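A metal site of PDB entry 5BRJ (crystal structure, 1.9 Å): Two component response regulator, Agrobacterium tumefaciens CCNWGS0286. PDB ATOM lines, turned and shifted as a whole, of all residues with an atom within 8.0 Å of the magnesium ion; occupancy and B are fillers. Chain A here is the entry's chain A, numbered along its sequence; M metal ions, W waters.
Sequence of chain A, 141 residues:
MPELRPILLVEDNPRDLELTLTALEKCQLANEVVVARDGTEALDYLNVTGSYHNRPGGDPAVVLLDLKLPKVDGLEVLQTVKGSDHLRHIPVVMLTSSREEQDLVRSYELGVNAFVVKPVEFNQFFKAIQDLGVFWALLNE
The backbone carbonyl oxygen of Asp 12 lies within hydrogen-bond range of the guanidinium group of Arg 37 (3.0 Å). NZ of Lys 118 lies within salt-bridge range of OD1 of Asp 66, 2.8 Å away. The backbone NH of Asp 66 sits at hydrogen-bond distance from the backbone carbonyl oxygen of Val 10 (3.0 Å). The side-chain amino group (NZ) of Lys 68 is in salt-bridge range of the side-chain carboxylate (OD2) of Asp 73. The side-chain carboxylate (OE2) of Glu 11 is in salt-bridge range of the side-chain amino group (NZ) of Lys 118 (2.7 Å). N of Asn 13 lies within hydrogen-bond range of OE1 of Glu 11, 2.9 Å away. The backbone carbonyl oxygen (O) of Glu 11 is in hydrogen-bond range of the guanidinium group (NE) of Arg 37, 2.9 Å away.
Residues that only touch the magnesium ion: Glu 11. Four residues have an atom within 4 Å of the magnesium ion: Glu 11, Asp 12, Asp 66 and Lys 68.
The magnesium ion is bound by the side-chain carboxylate (OD1) of Asp 12, the side-chain carboxylate (OD2) of Asp 66, water W2, water W1, water W3 and the backbone carbonyl oxygen (O) of Lys 68.
Water W1 bridges OD1 of Asp 66 (2.6 Å) and N of Lys 68 (3.1 Å). Water W2 lies within hydrogen-bond range of the side-chain carboxylate (OE1) of Glu 11 (2.6 Å), the side-chain amino group (NZ) of Lys 118 (3.2 Å) and the side-chain carboxylate (OD1) of Asp 66 (3.4 Å).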
ATOM      1  N   VAL A  10       2.403 -20.765 -31.026  1.00  0.00           N
ATOM      2  CA  VAL A  10       2.314 -21.920 -30.145  1.00  0.00           C
ATOM      3  C   VAL A  10       2.581 -21.446 -28.729  1.00  0.00           C
ATOM      4  O   VAL A  10       3.684 -21.023 -28.412  1.00  0.00           O
ATOM      5  CB  VAL A  10       3.307 -23.017 -30.512  1.00  0.00           C
ATOM      6  CG1 VAL A  10       3.014 -24.276 -29.702  1.00  0.00           C
ATOM      7  CG2 VAL A  10       3.252 -23.333 -32.007  1.00  0.00           C
ATOM      8  N   GLU A  11       1.572 -21.528 -27.864  1.00  0.00           N
ATOM      9  CA  GLU A  11       1.648 -20.932 -26.546  1.00  0.00           C
ATOM     10  C   GLU A  11       0.704 -21.616 -25.571  1.00  0.00           C
ATOM     11  O   GLU A  11      -0.495 -21.682 -25.842  1.00  0.00           O
ATOM     12  CB  GLU A  11       1.293 -19.443 -26.638  1.00  0.00           C
ATOM     13  CG  GLU A  11       1.210 -18.727 -25.283  1.00  0.00           C
ATOM     14  CD  GLU A  11       2.530 -18.739 -24.541  1.00  0.00           C
ATOM     15  OE1 GLU A  11       2.618 -19.387 -23.474  1.00  0.00           O
ATOM     16  OE2 GLU A  11       3.483 -18.079 -25.017  1.00  0.00           O
ATOM     17  N   ASP A  12       1.218 -22.078 -24.433  1.00  0.00           N
ATOM     18  CA  ASP A  12       0.359 -22.741 -23.449  1.00  0.00           C
ATOM     19  C   ASP A  12      -0.216 -21.803 -22.387  1.00  0.00           C
ATOM     20  O   ASP A  12      -1.276 -22.068 -21.837  1.00  0.00           O
ATOM     21  CB  ASP A  12       1.095 -23.914 -22.776  1.00  0.00           C
ATOM     22  CG  ASP A  12       2.345 -23.502 -21.999  1.00  0.00           C
ATOM     23  OD1 ASP A  12       3.147 -22.653 -22.461  1.00  0.00           O
ATOM     24  OD2 ASP A  12       2.552 -24.076 -20.893  1.00  0.00           O
ATOM     25  N   ASN A  13       0.479 -20.720 -22.078  1.00  0.00           N
ATOM     26  CA  ASN A  13      -0.015 -19.780 -21.061  1.00  0.00           C
ATOM     27  C   ASN A  13      -1.096 -18.866 -21.635  1.00  0.00           C
ATOM     28  O   ASN A  13      -0.832 -18.138 -22.598  1.00  0.00           O
ATOM     29  CB  ASN A  13       1.149 -18.971 -20.498  1.00  0.00           C
ATOM     30  CG  ASN A  13       0.738 -18.122 -19.293  1.00  0.00           C
ATOM     31  OD1 ASN A  13      -0.047 -17.201 -19.430  1.00  0.00           O
ATOM     32  ND2 ASN A  13       1.287 -18.446 -18.137  1.00  0.00           N
ATOM     33  N   ASP A  16      -0.131 -15.123 -21.709  1.00  0.00           N
ATOM     34  CA  ASP A  16       0.889 -14.909 -22.743  1.00  0.00           C
ATOM     35  C   ASP A  16       0.266 -15.000 -24.137  1.00  0.00           C
ATOM     36  O   ASP A  16       0.616 -14.207 -25.033  1.00  0.00           O
ATOM     37  CB  ASP A  16       2.041 -15.922 -22.595  1.00  0.00           C
ATOM     38  CG  ASP A  16       2.925 -15.612 -21.406  1.00  0.00           C
ATOM     39  OD1 ASP A  16       2.838 -14.487 -20.879  1.00  0.00           O
ATOM     40  OD2 ASP A  16       3.724 -16.482 -21.014  1.00  0.00           O
ATOM     41  N   ARG A  37      -1.966 -24.684 -28.625  1.00  0.00           N
ATOM     42  CA  ARG A  37      -1.778 -24.508 -27.192  1.00  0.00           C
ATOM     43  C   ARG A  37      -0.789 -25.477 -26.567  1.00  0.00           C
ATOM     44  O   ARG A  37      -0.435 -25.351 -25.388  1.00  0.00           O
ATOM     45  CB  ARG A  37      -3.142 -24.606 -26.483  1.00  0.00           C
ATOM     46  CG  ARG A  37      -4.155 -23.571 -26.950  1.00  0.00           C
ATOM     47  CD  ARG A  37      -3.656 -22.137 -26.730  1.00  0.00           C
ATOM     48  NE  ARG A  37      -3.354 -21.849 -25.323  1.00  0.00           N
ATOM     49  CZ  ARG A  37      -4.261 -21.532 -24.405  1.00  0.00           C
ATOM     50  NH1 ARG A  37      -5.543 -21.455 -24.732  1.00  0.00           N
ATOM     51  NH2 ARG A  37      -3.897 -21.289 -23.152  1.00  0.00           N
ATOM     52  N   LEU A  65       7.258 -19.887 -31.408  1.00  0.00           N
ATOM     53  CA  LEU A  65       7.220 -21.138 -30.627  1.00  0.00           C
ATOM     54  C   LEU A  65       7.651 -20.905 -29.185  1.00  0.00           C
ATOM     55  O   LEU A  65       8.838 -20.729 -28.898  1.00  0.00           O
ATOM     56  CB  LEU A  65       8.118 -22.199 -31.294  1.00  0.00           C
ATOM     57  CG  LEU A  65       8.216 -23.575 -30.622  1.00  0.00           C
ATOM     58  CD1 LEU A  65       6.832 -24.166 -30.377  1.00  0.00           C
ATOM     59  CD2 LEU A  65       9.043 -24.515 -31.500  1.00  0.00           C
ATOM     60  N   ASP A  66       6.690 -20.895 -28.289  1.00  0.00           N
ATOM     61  CA  ASP A  66       6.964 -20.805 -26.854  1.00  0.00           C
ATOM     62  C   ASP A  66       7.768 -22.033 -26.454  1.00  0.00           C
ATOM     63  O   ASP A  66       7.463 -23.137 -26.904  1.00  0.00           O
ATOM     64  CB  ASP A  66       5.647 -20.710 -26.080  1.00  0.00           C
ATOM     65  CG  ASP A  66       5.848 -20.769 -24.592  1.00  0.00           C
ATOM     66  OD1 ASP A  66       6.626 -19.952 -24.057  1.00  0.00           O
ATOM     67  OD2 ASP A  66       5.219 -21.635 -23.960  1.00  0.00           O
ATOM     68  N   LEU A  67       8.785 -21.850 -25.619  1.00  0.00           N
ATOM     69  CA  LEU A  67       9.767 -22.885 -25.339  1.00  0.00           C
ATOM     70  C   LEU A  67       9.248 -24.048 -24.473  1.00  0.00           C
ATOM     71  O   LEU A  67       9.597 -25.194 -24.696  1.00  0.00           O
ATOM     72  CB  LEU A  67      10.973 -22.268 -24.671  1.00  0.00           C
ATOM     73  CG  LEU A  67      12.108 -23.214 -24.278  1.00  0.00           C
ATOM     74  CD1 LEU A  67      12.646 -23.923 -25.518  1.00  0.00           C
ATOM     75  CD2 LEU A  67      13.195 -22.429 -23.559  1.00  0.00           C
ATOM     76  N   LYS A  68       8.436 -23.732 -23.465  1.00  0.00           N
ATOM     77  CA  LYS A  68       7.934 -24.754 -22.544  1.00  0.00           C
ATOM     78  C   LYS A  68       6.471 -25.039 -22.805  1.00  0.00           C
ATOM     79  O   LYS A  68       5.638 -24.131 -22.719  1.00  0.00           O
ATOM     80  CB  LYS A  68       8.144 -24.327 -21.091  1.00  0.00           C
ATOM     81  CG  LYS A  68       9.587 -24.008 -20.699  1.00  0.00           C
ATOM     82  CD  LYS A  68      10.519 -25.207 -20.925  1.00  0.00           C
ATOM     83  CE  LYS A  68      10.002 -26.456 -20.221  1.00  0.00           C
ATOM     84  NZ  LYS A  68      10.782 -27.668 -20.581  1.00  0.00           N
ATOM     85  N   LEU A  69       6.138 -26.277 -23.151  1.00  0.00           N
ATOM     86  CA  LEU A  69       4.773 -26.657 -23.442  1.00  0.00           C
ATOM     87  C   LEU A  69       4.442 -27.998 -22.791  1.00  0.00           C
ATOM     88  O   LEU A  69       5.338 -28.817 -22.595  1.00  0.00           O
ATOM     89  CB  LEU A  69       4.550 -26.748 -24.965  1.00  0.00           C
ATOM     90  CG  LEU A  69       4.900 -25.579 -25.881  1.00  0.00           C
ATOM     91  CD1 LEU A  69       4.927 -26.081 -27.314  1.00  0.00           C
ATOM     92  CD2 LEU A  69       3.862 -24.473 -25.735  1.00  0.00           C
ATOM     93  N   PRO A  70       3.173 -28.247 -22.490  1.00  0.00           N
ATOM     94  CA  PRO A  70       2.816 -29.579 -21.980  1.00  0.00           C
ATOM     95  C   PRO A  70       2.695 -30.589 -23.125  1.00  0.00           C
ATOM     96  O   PRO A  70       2.600 -30.176 -24.281  1.00  0.00           O
ATOM     97  CB  PRO A  70       1.475 -29.348 -21.287  1.00  0.00           C
ATOM     98  CG  PRO A  70       0.875 -28.193 -21.998  1.00  0.00           C
ATOM     99  CD  PRO A  70       2.034 -27.311 -22.430  1.00  0.00           C
ATOM    100  N   ASP A  73       6.978 -30.940 -25.630  1.00  0.00           N
ATOM    101  CA  ASP A  73       7.652 -29.723 -25.208  1.00  0.00           C
ATOM    102  C   ASP A  73       8.037 -28.867 -26.417  1.00  0.00           C
ATOM    103  O   ASP A  73       8.113 -29.365 -27.549  1.00  0.00           O
ATOM    104  CB  ASP A  73       8.886 -30.067 -24.391  1.00  0.00           C
ATOM    105  CG  ASP A  73       9.337 -28.926 -23.513  1.00  0.00           C
ATOM    106  OD1 ASP A  73       8.541 -27.981 -23.313  1.00  0.00           O
ATOM    107  OD2 ASP A  73      10.480 -28.991 -23.013  1.00  0.00           O
ATOM    108  N   GLY A  74       8.268 -27.571 -26.194  1.00  0.00           N
ATOM    109  CA  GLY A  74       8.622 -26.689 -27.288  1.00  0.00           C
ATOM    110  C   GLY A  74       9.889 -27.125 -27.983  1.00  0.00           C
ATOM    111  O   GLY A  74       9.980 -27.090 -29.212  1.00  0.00           O
ATOM    112  N   LEU A  95      10.062 -18.267 -28.368  1.00  0.00           N
ATOM    113  CA  LEU A  95       9.630 -17.347 -27.321  1.00  0.00           C
ATOM    114  C   LEU A  95      10.072 -17.868 -25.976  1.00  0.00           C
ATOM    115  O   LEU A  95       9.842 -19.027 -25.646  1.00  0.00           O
ATOM    116  CB  LEU A  95       8.113 -17.174 -27.325  1.00  0.00           C
ATOM    117  CG  LEU A  95       7.451 -16.855 -28.673  1.00  0.00           C
ATOM    118  CD1 LEU A  95       5.971 -16.717 -28.440  1.00  0.00           C
ATOM    119  CD2 LEU A  95       8.044 -15.601 -29.278  1.00  0.00           C
ATOM    120  N   THR A  96      10.726 -17.016 -25.184  1.00  0.00           N
ATOM    121  CA  THR A  96      11.155 -17.424 -23.852  1.00  0.00           C
ATOM    122  C   THR A  96      10.749 -16.395 -22.807  1.00  0.00           C
ATOM    123  O   THR A  96      10.333 -15.282 -23.136  1.00  0.00           O
ATOM    124  CB  THR A  96      12.671 -17.637 -23.791  1.00  0.00           C
ATOM    125  OG1 THR A  96      13.335 -16.378 -23.771  1.00  0.00           O
ATOM    126  CG2 THR A  96      13.167 -18.468 -24.974  1.00  0.00           C
ATOM    127  N   SER A  97      10.849 -16.789 -21.532  1.00  0.00           N
ATOM    128  CA  SER A  97      10.566 -15.900 -20.410  1.00  0.00           C
ATOM    129  C   SER A  97      11.826 -15.175 -19.932  1.00  0.00           C
ATOM    130  O   SER A  97      11.756 -14.129 -19.293  1.00  0.00           O
ATOM    131  CB  SER A  97       9.964 -16.698 -19.239  1.00  0.00           C
ATOM    132  OG  SER A  97       8.733 -17.312 -19.602  1.00  0.00           O
ATOM    133  N   GLU A 101      17.140 -18.727 -20.716  1.00  0.00           N
ATOM    134  CA  GLU A 101      16.529 -19.833 -21.429  1.00  0.00           C
ATOM    135  C   GLU A 101      17.071 -19.889 -22.851  1.00  0.00           C
ATOM    136  O   GLU A 101      17.186 -20.962 -23.433  1.00  0.00           O
ATOM    137  CB  GLU A 101      15.000 -19.708 -21.456  1.00  0.00           C
ATOM    138  CG  GLU A 101      14.310 -19.961 -20.132  1.00  0.00           C
ATOM    139  CD  GLU A 101      12.806 -19.961 -20.293  1.00  0.00           C
ATOM    140  OE1 GLU A 101      12.309 -19.124 -21.069  1.00  0.00           O
ATOM    141  OE2 GLU A 101      12.120 -20.785 -19.650  1.00  0.00           O
ATOM    142  N   LYS A 118       9.462 -12.690 -23.728  1.00  0.00           N
ATOM    143  CA  LYS A 118       8.119 -12.210 -23.469  1.00  0.00           C
ATOM    144  C   LYS A 118       8.144 -11.125 -22.378  1.00  0.00           C
ATOM    145  O   LYS A 118       9.044 -11.121 -21.538  1.00  0.00           O
ATOM    146  CB  LYS A 118       7.200 -13.385 -23.081  1.00  0.00           C
ATOM    147  CG  LYS A 118       7.018 -14.381 -24.228  1.00  0.00           C
ATOM    148  CD  LYS A 118       5.920 -15.394 -23.939  1.00  0.00           C
ATOM    149  CE  LYS A 118       6.492 -16.716 -23.462  1.00  0.00           C
ATOM    150  NZ  LYS A 118       5.389 -17.679 -23.113  1.00  0.00           N
HETATM  151 MG    MG M   1       4.985 -22.142 -22.097  1.00  0.00          MG
HETATM  152  O   HOH W   1       6.999 -21.434 -21.996  1.00  0.00           O
HETATM  153  O   HOH W   2       4.211 -20.223 -21.657  1.00  0.00           O
HETATM  154  O   HOH W   3       4.655 -22.890 -20.111  1.00  0.00           O
